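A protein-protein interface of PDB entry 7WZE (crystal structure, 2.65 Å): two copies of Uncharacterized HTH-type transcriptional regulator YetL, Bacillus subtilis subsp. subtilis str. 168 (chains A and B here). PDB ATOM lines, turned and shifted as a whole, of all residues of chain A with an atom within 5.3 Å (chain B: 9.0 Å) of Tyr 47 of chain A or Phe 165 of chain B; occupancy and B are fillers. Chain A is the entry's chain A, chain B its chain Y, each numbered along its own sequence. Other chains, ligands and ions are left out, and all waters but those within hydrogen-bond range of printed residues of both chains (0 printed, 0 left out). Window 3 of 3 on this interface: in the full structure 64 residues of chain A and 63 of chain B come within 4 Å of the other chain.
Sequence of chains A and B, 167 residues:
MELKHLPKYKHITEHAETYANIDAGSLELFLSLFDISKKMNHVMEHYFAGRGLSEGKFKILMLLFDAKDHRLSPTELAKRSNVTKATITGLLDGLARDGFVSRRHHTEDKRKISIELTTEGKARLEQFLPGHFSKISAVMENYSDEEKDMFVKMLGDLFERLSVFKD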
ATOM      1  N   VAL A  43     -16.942 -22.442   1.450  1.00  0.00           N
ATOM      2  CA  VAL A  43     -16.801 -22.986   2.793  1.00  0.00           C
ATOM      3  C   VAL A  43     -18.051 -22.707   3.622  1.00  0.00           C
ATOM      4  O   VAL A  43     -18.534 -23.581   4.354  1.00  0.00           O
ATOM      5  CB  VAL A  43     -15.538 -22.417   3.460  1.00  0.00           C
ATOM      6  CG1 VAL A  43     -15.480 -22.866   4.844  1.00  0.00           C
ATOM      7  CG2 VAL A  43     -14.310 -22.909   2.751  1.00  0.00           C
ATOM      8  N   MET A  44     -18.618 -21.512   3.491  1.00  0.00           N
ATOM      9  CA  MET A  44     -19.743 -21.106   4.340  1.00  0.00           C
ATOM     10  C   MET A  44     -21.002 -21.897   4.065  1.00  0.00           C
ATOM     11  O   MET A  44     -21.728 -22.259   4.998  1.00  0.00           O
ATOM     12  CB  MET A  44     -20.049 -19.618   4.177  1.00  0.00           C
ATOM     13  CG  MET A  44     -19.061 -18.699   4.866  1.00  0.00           C
ATOM     14  SD  MET A  44     -18.591 -19.250   6.694  1.00  0.00           S
ATOM     15  CE  MET A  44     -16.851 -18.404   6.786  1.00  0.00           C
ATOM     16  N   GLU A  45     -21.278 -22.167   2.789  1.00  0.00           N
ATOM     17  CA  GLU A  45     -22.499 -22.899   2.474  1.00  0.00           C
ATOM     18  C   GLU A  45     -22.488 -24.283   3.125  1.00  0.00           C
ATOM     19  O   GLU A  45     -23.519 -24.744   3.631  1.00  0.00           O
ATOM     20  CB  GLU A  45     -22.699 -22.978   0.957  1.00  0.00           C
ATOM     21  CG  GLU A  45     -23.045 -21.614   0.317  1.00  0.00           C
ATOM     22  CD  GLU A  45     -24.448 -21.548  -0.300  1.00  0.00           C
ATOM     23  OE1 GLU A  45     -24.966 -22.603  -0.730  1.00  0.00           O
ATOM     24  OE2 GLU A  45     -25.034 -20.435  -0.355  1.00  0.00           O
ATOM     25  N   HIS A  46     -21.317 -24.935   3.183  1.00  0.00           N
ATOM     26  CA  HIS A  46     -21.260 -26.274   3.773  1.00  0.00           C
ATOM     27  C   HIS A  46     -21.228 -26.230   5.303  1.00  0.00           C
ATOM     28  O   HIS A  46     -21.811 -27.099   5.961  1.00  0.00           O
ATOM     29  CB  HIS A  46     -20.051 -27.053   3.236  1.00  0.00           C
ATOM     30  CG  HIS A  46     -20.108 -27.335   1.762  1.00  0.00           C
ATOM     31  ND1 HIS A  46     -21.165 -27.994   1.166  1.00  0.00           N
ATOM     32  CD2 HIS A  46     -19.231 -27.059   0.767  1.00  0.00           C
ATOM     33  CE1 HIS A  46     -20.940 -28.100  -0.132  1.00  0.00           C
ATOM     34  NE2 HIS A  46     -19.774 -27.540  -0.400  1.00  0.00           N
ATOM     35  N   TYR A  47     -20.544 -25.241   5.882  1.00  0.00           N
ATOM     36  CA  TYR A  47     -20.552 -25.049   7.331  1.00  0.00           C
ATOM     37  C   TYR A  47     -21.977 -24.976   7.886  1.00  0.00           C
ATOM     38  O   TYR A  47     -22.356 -25.752   8.773  1.00  0.00           O
ATOM     39  CB  TYR A  47     -19.746 -23.793   7.673  1.00  0.00           C
ATOM     40  CG  TYR A  47     -19.762 -23.336   9.123  1.00  0.00           C
ATOM     41  CD1 TYR A  47     -19.106 -24.069  10.141  1.00  0.00           C
ATOM     42  CD2 TYR A  47     -20.351 -22.131   9.459  1.00  0.00           C
ATOM     43  CE1 TYR A  47     -19.104 -23.615  11.465  1.00  0.00           C
ATOM     44  CE2 TYR A  47     -20.348 -21.663  10.754  1.00  0.00           C
ATOM     45  CZ  TYR A  47     -19.731 -22.402  11.757  1.00  0.00           C
ATOM     46  OH  TYR A  47     -19.759 -21.894  13.042  1.00  0.00           O
ATOM     47  N   PHE A  48     -22.786 -24.050   7.369  1.00  0.00           N
ATOM     48  CA  PHE A  48     -24.164 -23.970   7.834  1.00  0.00           C
ATOM     49  C   PHE A  48     -24.960 -25.210   7.452  1.00  0.00           C
ATOM     50  O   PHE A  48     -25.931 -25.550   8.137  1.00  0.00           O
ATOM     51  CB  PHE A  48     -24.856 -22.724   7.277  1.00  0.00           C
ATOM     52  CG  PHE A  48     -24.302 -21.432   7.805  1.00  0.00           C
ATOM     53  CD1 PHE A  48     -24.373 -21.136   9.154  1.00  0.00           C
ATOM     54  CD2 PHE A  48     -23.760 -20.495   6.950  1.00  0.00           C
ATOM     55  CE1 PHE A  48     -23.879 -19.944   9.653  1.00  0.00           C
ATOM     56  CE2 PHE A  48     -23.267 -19.304   7.442  1.00  0.00           C
ATOM     57  CZ  PHE A  48     -23.334 -19.029   8.806  1.00  0.00           C
ATOM     58  N   ALA A  49     -24.595 -25.877   6.356  1.00  0.00           N
ATOM     59  CA  ALA A  49     -25.242 -27.140   6.024  1.00  0.00           C
ATOM     60  C   ALA A  49     -24.972 -28.185   7.094  1.00  0.00           C
ATOM     61  O   ALA A  49     -25.883 -28.913   7.511  1.00  0.00           O
ATOM     62  CB  ALA A  49     -24.766 -27.633   4.658  1.00  0.00           C
ATOM     63  N   GLY A  50     -23.733 -28.239   7.581  1.00  0.00           N
ATOM     64  CA  GLY A  50     -23.333 -29.163   8.622  1.00  0.00           C
ATOM     65  C   GLY A  50     -24.213 -29.067   9.845  1.00  0.00           C
ATOM     66  O   GLY A  50     -24.214 -29.950  10.708  1.00  0.00           O
ATOM     67  N   ARG A  51     -24.966 -27.980   9.929  1.00  0.00           N
ATOM     68  CA  ARG A  51     -25.866 -27.745  11.044  1.00  0.00           C
ATOM     69  C   ARG A  51     -27.323 -27.729  10.602  1.00  0.00           C
ATOM     70  O   ARG A  51     -28.183 -27.265  11.356  1.00  0.00           O
ATOM     71  CB  ARG A  51     -25.512 -26.422  11.729  1.00  0.00           C
ATOM     72  CG  ARG A  51     -24.118 -26.367  12.336  1.00  0.00           C
ATOM     73  CD  ARG A  51     -23.963 -27.337  13.499  1.00  0.00           C
ATOM     74  NE  ARG A  51     -22.954 -26.866  14.442  1.00  0.00           N
ATOM     75  CZ  ARG A  51     -22.603 -27.511  15.547  1.00  0.00           C
ATOM     76  NH1 ARG A  51     -23.178 -28.669  15.856  1.00  0.00           N
ATOM     77  NH2 ARG A  51     -21.676 -26.995  16.343  1.00  0.00           N
ATOM     78  N   PHE A 128     -24.297 -23.616  19.646  1.00  0.00           N
ATOM     79  CA  PHE A 128     -23.541 -23.423  18.417  1.00  0.00           C
ATOM     80  C   PHE A 128     -22.674 -22.167  18.428  1.00  0.00           C
ATOM     81  O   PHE A 128     -21.533 -22.203  17.943  1.00  0.00           O
ATOM     82  CB  PHE A 128     -24.505 -23.383  17.230  1.00  0.00           C
ATOM     83  CG  PHE A 128     -23.897 -22.819  15.984  1.00  0.00           C
ATOM     84  CD1 PHE A 128     -22.902 -23.504  15.313  1.00  0.00           C
ATOM     85  CD2 PHE A 128     -24.331 -21.603  15.488  1.00  0.00           C
ATOM     86  CE1 PHE A 128     -22.338 -22.985  14.173  1.00  0.00           C
ATOM     87  CE2 PHE A 128     -23.777 -21.072  14.351  1.00  0.00           C
ATOM     88  CZ  PHE A 128     -22.778 -21.767  13.684  1.00  0.00           C
ATOM     89  N   GLY A 131     -18.518 -21.924  19.328  1.00  0.00           N
ATOM     90  CA  GLY A 131     -17.597 -22.369  18.305  1.00  0.00           C
ATOM     91  C   GLY A 131     -17.599 -21.452  17.102  1.00  0.00           C
ATOM     92  O   GLY A 131     -16.565 -21.241  16.474  1.00  0.00           O
ATOM     93  N   HIS A 132     -18.753 -20.884  16.781  1.00  0.00           N
ATOM     94  CA  HIS A 132     -18.816 -19.994  15.629  1.00  0.00           C
ATOM     95  C   HIS A 132     -17.985 -18.737  15.865  1.00  0.00           C
ATOM     96  O   HIS A 132     -17.282 -18.274  14.959  1.00  0.00           O
ATOM     97  CB  HIS A 132     -20.281 -19.648  15.334  1.00  0.00           C
ATOM     98  CG  HIS A 132     -20.473 -18.760  14.139  1.00  0.00           C
ATOM     99  ND1 HIS A 132     -20.342 -19.211  12.844  1.00  0.00           N
ATOM    100  CD2 HIS A 132     -20.810 -17.453  14.049  1.00  0.00           C
ATOM    101  CE1 HIS A 132     -20.576 -18.215  12.009  1.00  0.00           C
ATOM    102  NE2 HIS A 132     -20.858 -17.138  12.715  1.00  0.00           N
ATOM    103  N   LYS A 135     -14.052 -19.584  15.826  1.00  0.00           N
ATOM    104  CA  LYS A 135     -13.510 -19.694  14.473  1.00  0.00           C
ATOM    105  C   LYS A 135     -13.302 -18.324  13.841  1.00  0.00           C
ATOM    106  O   LYS A 135     -12.284 -18.087  13.175  1.00  0.00           O
ATOM    107  CB  LYS A 135     -14.423 -20.563  13.602  1.00  0.00           C
ATOM    108  CG  LYS A 135     -14.669 -21.928  14.202  1.00  0.00           C
ATOM    109  CD  LYS A 135     -15.583 -22.814  13.375  1.00  0.00           C
ATOM    110  CE  LYS A 135     -15.732 -24.165  14.074  1.00  0.00           C
ATOM    111  NZ  LYS A 135     -16.673 -25.086  13.394  1.00  0.00           N
ATOM    112  N   ILE A 136     -14.257 -17.406  14.020  1.00  0.00           N
ATOM    113  CA  ILE A 136     -14.084 -16.070  13.470  1.00  0.00           C
ATOM    114  C   ILE A 136     -12.894 -15.384  14.121  1.00  0.00           C
ATOM    115  O   ILE A 136     -12.032 -14.808  13.443  1.00  0.00           O
ATOM    116  CB  ILE A 136     -15.382 -15.257  13.614  1.00  0.00           C
ATOM    117  CG1 ILE A 136     -16.434 -15.749  12.606  1.00  0.00           C
ATOM    118  CG2 ILE A 136     -15.111 -13.763  13.464  1.00  0.00           C
ATOM    119  CD1 ILE A 136     -17.867 -15.319  12.973  1.00  0.00           C
ATOM    120  N   VAL A 139      -9.766 -16.366  12.562  1.00  0.00           N
ATOM    121  CA  VAL A 139      -9.460 -15.808  11.250  1.00  0.00           C
ATOM    122  C   VAL A 139      -8.795 -14.436  11.371  1.00  0.00           C
ATOM    123  O   VAL A 139      -7.828 -14.139  10.661  1.00  0.00           O
ATOM    124  CB  VAL A 139     -10.733 -15.768  10.396  1.00  0.00           C
ATOM    125  CG1 VAL A 139     -10.470 -15.065   9.075  1.00  0.00           C
ATOM    126  CG2 VAL A 139     -11.228 -17.179  10.173  1.00  0.00           C
ATOM    127  N   ILE B  22     -15.385 -12.031  21.497  1.00  0.00           N
ATOM    128  CA  ILE B  22     -15.229 -11.652  20.098  1.00  0.00           C
ATOM    129  C   ILE B  22     -14.931 -10.156  20.029  1.00  0.00           C
ATOM    130  O   ILE B  22     -15.529  -9.364  20.765  1.00  0.00           O
ATOM    131  CB  ILE B  22     -16.476 -12.018  19.268  1.00  0.00           C
ATOM    132  CG1 ILE B  22     -16.228 -11.762  17.782  1.00  0.00           C
ATOM    133  CG2 ILE B  22     -17.705 -11.259  19.747  1.00  0.00           C
ATOM    134  CD1 ILE B  22     -15.402 -12.811  17.106  1.00  0.00           C
ATOM    135  N   LEU B  27     -15.113  -9.043  14.184  1.00  0.00           N
ATOM    136  CA  LEU B  27     -16.458  -9.415  13.755  1.00  0.00           C
ATOM    137  C   LEU B  27     -16.919  -8.541  12.588  1.00  0.00           C
ATOM    138  O   LEU B  27     -17.466  -9.045  11.595  1.00  0.00           O
ATOM    139  CB  LEU B  27     -17.412  -9.317  14.935  1.00  0.00           C
ATOM    140  CG  LEU B  27     -18.747 -10.061  14.965  1.00  0.00           C
ATOM    141  CD1 LEU B  27     -19.874  -9.063  14.851  1.00  0.00           C
ATOM    142  CD2 LEU B  27     -18.858 -11.087  13.885  1.00  0.00           C
ATOM    143  N   PHE B  30     -15.193  -9.544   9.404  1.00  0.00           N
ATOM    144  CA  PHE B  30     -15.622 -10.825   8.881  1.00  0.00           C
ATOM    145  C   PHE B  30     -16.980 -10.711   8.210  1.00  0.00           C
ATOM    146  O   PHE B  30     -17.231 -11.357   7.188  1.00  0.00           O
ATOM    147  CB  PHE B  30     -15.653 -11.838  10.019  1.00  0.00           C
ATOM    148  CG  PHE B  30     -16.004 -13.213   9.592  1.00  0.00           C
ATOM    149  CD1 PHE B  30     -15.038 -14.049   9.069  1.00  0.00           C
ATOM    150  CD2 PHE B  30     -17.308 -13.669   9.700  1.00  0.00           C
ATOM    151  CE1 PHE B  30     -15.366 -15.339   8.682  1.00  0.00           C
ATOM    152  CE2 PHE B  30     -17.649 -14.936   9.311  1.00  0.00           C
ATOM    153  CZ  PHE B  30     -16.674 -15.779   8.805  1.00  0.00           C
ATOM    154  N   PHE B  34     -17.898 -11.124   4.281  1.00  0.00           N
ATOM    155  CA  PHE B  34     -18.900 -12.053   3.794  1.00  0.00           C
ATOM    156  C   PHE B  34     -19.910 -11.350   2.902  1.00  0.00           C
ATOM    157  O   PHE B  34     -20.330 -11.913   1.888  1.00  0.00           O
ATOM    158  CB  PHE B  34     -19.577 -12.746   4.973  1.00  0.00           C
ATOM    159  CG  PHE B  34     -20.531 -13.838   4.575  1.00  0.00           C
ATOM    160  CD1 PHE B  34     -21.759 -13.963   5.191  1.00  0.00           C
ATOM    161  CD2 PHE B  34     -20.179 -14.770   3.620  1.00  0.00           C
ATOM    162  CE1 PHE B  34     -22.634 -14.978   4.841  1.00  0.00           C
ATOM    163  CE2 PHE B  34     -21.058 -15.790   3.271  1.00  0.00           C
ATOM    164  CZ  PHE B  34     -22.284 -15.886   3.888  1.00  0.00           C
ATOM    165  N   LEU B 158      -6.232 -14.641   5.462  1.00  0.00           N
ATOM    166  CA  LEU B 158      -7.646 -15.005   5.554  1.00  0.00           C
ATOM    167  C   LEU B 158      -7.975 -16.171   4.643  1.00  0.00           C
ATOM    168  O   LEU B 158      -8.833 -17.001   4.973  1.00  0.00           O
ATOM    169  CB  LEU B 158      -8.563 -13.825   5.228  1.00  0.00           C
ATOM    170  CG  LEU B 158      -8.630 -12.570   6.107  1.00  0.00           C
ATOM    171  CD1 LEU B 158      -7.727 -12.678   7.338  1.00  0.00           C
ATOM    172  CD2 LEU B 158      -8.383 -11.273   5.318  1.00  0.00           C
ATOM    173  N   PHE B 159      -7.347 -16.226   3.471  1.00  0.00           N
ATOM    174  CA  PHE B 159      -7.643 -17.315   2.553  1.00  0.00           C
ATOM    175  C   PHE B 159      -7.358 -18.668   3.190  1.00  0.00           C
ATOM    176  O   PHE B 159      -8.162 -19.597   3.067  1.00  0.00           O
ATOM    177  CB  PHE B 159      -6.868 -17.149   1.249  1.00  0.00           C
ATOM    178  CG  PHE B 159      -7.338 -18.068   0.155  1.00  0.00           C
ATOM    179  CD1 PHE B 159      -8.355 -17.690  -0.703  1.00  0.00           C
ATOM    180  CD2 PHE B 159      -6.775 -19.326   0.000  1.00  0.00           C
ATOM    181  CE1 PHE B 159      -8.789 -18.550  -1.706  1.00  0.00           C
ATOM    182  CE2 PHE B 159      -7.207 -20.186  -0.989  1.00  0.00           C
ATOM    183  CZ  PHE B 159      -8.211 -19.804  -1.844  1.00  0.00           C
ATOM    184  N   GLU B 160      -6.218 -18.806   3.866  1.00  0.00           N
ATOM    185  CA  GLU B 160      -5.898 -20.102   4.440  1.00  0.00           C
ATOM    186  C   GLU B 160      -6.729 -20.382   5.680  1.00  0.00           C
ATOM    187  O   GLU B 160      -7.137 -21.528   5.895  1.00  0.00           O
ATOM    188  CB  GLU B 160      -4.404 -20.200   4.775  1.00  0.00           C
ATOM    189  CG  GLU B 160      -3.986 -19.629   6.127  1.00  0.00           C
ATOM    190  CD  GLU B 160      -2.489 -19.701   6.382  1.00  0.00           C
ATOM    191  OE1 GLU B 160      -1.729 -19.896   5.413  1.00  0.00           O
ATOM    192  OE2 GLU B 160      -2.078 -19.562   7.555  1.00  0.00           O
ATOM    193  N   ARG B 161      -7.028 -19.356   6.474  1.00  0.00           N
ATOM    194  CA  ARG B 161      -7.668 -19.591   7.758  1.00  0.00           C
ATOM    195  C   ARG B 161      -9.140 -19.921   7.615  1.00  0.00           C
ATOM    196  O   ARG B 161      -9.707 -20.530   8.527  1.00  0.00           O
ATOM    197  CB  ARG B 161      -7.458 -18.390   8.691  1.00  0.00           C
ATOM    198  CG  ARG B 161      -5.975 -18.175   9.012  1.00  0.00           C
ATOM    199  CD  ARG B 161      -5.654 -16.925   9.832  1.00  0.00           C
ATOM    200  NE  ARG B 161      -4.201 -16.831  10.005  1.00  0.00           N
ATOM    201  CZ  ARG B 161      -3.514 -17.359  11.021  1.00  0.00           C
ATOM    202  NH1 ARG B 161      -4.141 -18.009  11.997  1.00  0.00           N
ATOM    203  NH2 ARG B 161      -2.191 -17.231  11.067  1.00  0.00           N
ATOM    204  N   LEU B 162      -9.745 -19.605   6.465  1.00  0.00           N
ATOM    205  CA  LEU B 162     -11.128 -19.982   6.196  1.00  0.00           C
ATOM    206  C   LEU B 162     -11.304 -21.490   6.234  1.00  0.00           C
ATOM    207  O   LEU B 162     -12.416 -21.967   6.471  1.00  0.00           O
ATOM    208  CB  LEU B 162     -11.563 -19.456   4.819  1.00  0.00           C
ATOM    209  CG  LEU B 162     -12.333 -18.157   4.556  1.00  0.00           C
ATOM    210  CD1 LEU B 162     -12.197 -17.127   5.666  1.00  0.00           C
ATOM    211  CD2 LEU B 162     -11.842 -17.592   3.226  1.00  0.00           C
ATOM    212  N   SER B 163     -10.221 -22.244   6.064  1.00  0.00           N
ATOM    213  CA  SER B 163     -10.301 -23.696   6.137  1.00  0.00           C
ATOM    214  C   SER B 163     -10.887 -24.152   7.465  1.00  0.00           C
ATOM    215  O   SER B 163     -11.525 -25.209   7.525  1.00  0.00           O
ATOM    216  CB  SER B 163      -8.914 -24.305   5.916  1.00  0.00           C
ATOM    217  OG  SER B 163      -8.481 -24.073   4.582  1.00  0.00           O
ATOM    218  N   VAL B 164     -10.681 -23.379   8.534  1.00  0.00           N
ATOM    219  CA  VAL B 164     -11.211 -23.752   9.842  1.00  0.00           C
ATOM    220  C   VAL B 164     -12.737 -23.772   9.863  1.00  0.00           C
ATOM    221  O   VAL B 164     -13.330 -24.308  10.802  1.00  0.00           O
ATOM    222  CB  VAL B 164     -10.697 -22.823  10.960  1.00  0.00           C
ATOM    223  CG1 VAL B 164     -11.507 -21.563  11.022  1.00  0.00           C
ATOM    224  CG2 VAL B 164     -10.766 -23.525  12.290  1.00  0.00           C
ATOM    225  N   PHE B 165     -13.412 -23.200   8.873  1.00  0.00           N
ATOM    226  CA  PHE B 165     -14.859 -23.386   8.860  1.00  0.00           C
ATOM    227  C   PHE B 165     -15.278 -24.755   8.321  1.00  0.00           C
ATOM    228  O   PHE B 165     -16.441 -24.937   7.941  1.00  0.00           O
ATOM    229  CB  PHE B 165     -15.531 -22.232   8.096  1.00  0.00           C
ATOM    230  CG  PHE B 165     -15.531 -20.945   8.865  1.00  0.00           C
ATOM    231  CD1 PHE B 165     -16.492 -20.712   9.850  1.00  0.00           C
ATOM    232  CD2 PHE B 165     -14.546 -20.004   8.660  1.00  0.00           C
ATOM    233  CE1 PHE B 165     -16.481 -19.552  10.583  1.00  0.00           C
ATOM    234  CE2 PHE B 165     -14.526 -18.850   9.393  1.00  0.00           C
ATOM    235  CZ  PHE B 165     -15.499 -18.621  10.356  1.00  0.00           C
ATOM    236  N   LYS B 166     -14.352 -25.704   8.232  1.00  0.00           N
ATOM    237  CA  LYS B 166     -14.728 -27.101   8.035  1.00  0.00           C
ATOM    238  C   LYS B 166     -15.256 -27.635   9.364  1.00  0.00           C
ATOM    239  O   LYS B 166     -14.474 -28.047  10.228  1.00  0.00           O
ATOM    240  CB  LYS B 166     -13.555 -27.923   7.527  1.00  0.00           C
ATOM    241  CG  LYS B 166     -13.997 -28.971   6.515  1.00  0.00           C
ATOM    242  CD  LYS B 166     -14.819 -30.093   7.154  1.00  0.00           C
ATOM    243  CE  LYS B 166     -13.915 -31.082   7.859  1.00  0.00           C
ATOM    244  NZ  LYS B 166     -12.936 -31.646   6.899  1.00  0.00           N
ATOM    245  N   ASP B 167     -16.581 -27.652   9.530  1.00  0.00           N
ATOM    246  CA  ASP B 167     -17.187 -28.124  10.780  1.00  0.00           C
ATOM    247  C   ASP B 167     -17.040 -29.647  10.935  1.00  0.00           C
ATOM    248  O   ASP B 167     -17.934 -30.420  10.575  1.00  0.00           O
ATOM    249  CB  ASP B 167     -18.667 -27.714  10.853  1.00  0.00           C
ATOM    250  CG  ASP B 167     -19.066 -27.148  12.225  1.00  0.00           C
ATOM    251  OD1 ASP B 167     -18.221 -27.127  13.143  1.00  0.00           O
ATOM    252  OD2 ASP B 167     -20.232 -26.718  12.379  1.00  0.00           O
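Of the 15 printed residues of chain A, 7 touch a printed residue of chain B. Printed residues of chain A that touch a printed residue of chain B: Val 43, Met 44, Tyr 47, Arg 51, Lys 135, Ile 136 and Val 139. Along chain A the printed residues that touch a printed residue of chain B span positions 43 to 139. Along chain B the printed residues that touch a printed residue of chain A span positions 22 to 167.
Of chain B, only Phe 165 (3.5 Å) and Asp 167 (3.4 Å) come within 4 Å of Tyr 47 of chain A. Of chain A, only Val 43, Met 44, Tyr 47, Lys 135, Ile 136 and Val 139 come within 4 Å of Phe 165 of chain B. No residue of chain B comes within 4 Å of His 132 of chain A. Printed residues of chain A within 4 Å of Val 164 of chain B: Lys 135 (3.7 Å). Of the printed residues of chain A, Leu 158 of chain B touches Val 139. Ala 49 of chain A touches none of the printed residues of chain B. The nearest residue of chain B that does not touch Tyr 47 of chain A is Lys 166 of chain B (5.3 Å). The nearest residue of chain A that does not touch Phe 165 of chain B is His 132 of chain A (4.5 Å).
The side-chain hydroxyl (OH) of Tyr 47 of chain A is in hydrogen-bond range of a ring nitrogen (ND1) of His 132 of chain A.
The side-chain amino group of Lys 135 of chain A lies within salt-bridge range of the side-chain carboxylate of Asp 167 of chain B, 2.6 Å away. The guanidinium group of Arg 51 of chain A lies within salt-bridge range of the side-chain carboxylate of Asp 167 of chain B, at 3.4 Å.
Among the printed residues, pairs that only touch across the chains: Val 43 of chain A with Leu 162 of chain B (3.6 Å), Val 43 of chain A with Phe 165 of chain B (3.3 Å), Met 44 of chain A with Phe 30 of chain B (3.3 Å), Met 44 of chain A with Phe 34 of chain B (3.9 Å), Met 44 of chain A with Phe 165 of chain B (3.4 Å), Tyr 47 of chain A with Phe 165 of chain B (3.5 Å), Tyr 47 of chain A with Asp 167 of chain B (3.4 Å), Lys 135 of chain A with Val 164 of chain B (3.7 Å), Lys 135 of chain A with Phe 165 of chain B (3.8 Å), Ile 136 of chain A with Ile 22 of chain B (3.8 Å), Ile 136 of chain A with Phe 30 of chain B (3.6 Å), Ile 136 of chain A with Phe 165 of chain B (3.8 Å), Val 139 of chain A with Leu 158 of chain B (3.6 Å), Val 139 of chain A with Arg 161 of chain B (3.6 Å) and Val 139 of chain A with Phe 165 of chain B (3.8 Å).
No position is printed for both chains. Of the 17 pairs that touch across the chains among the printed residues, none has its exchanged pair printed and touching as well.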
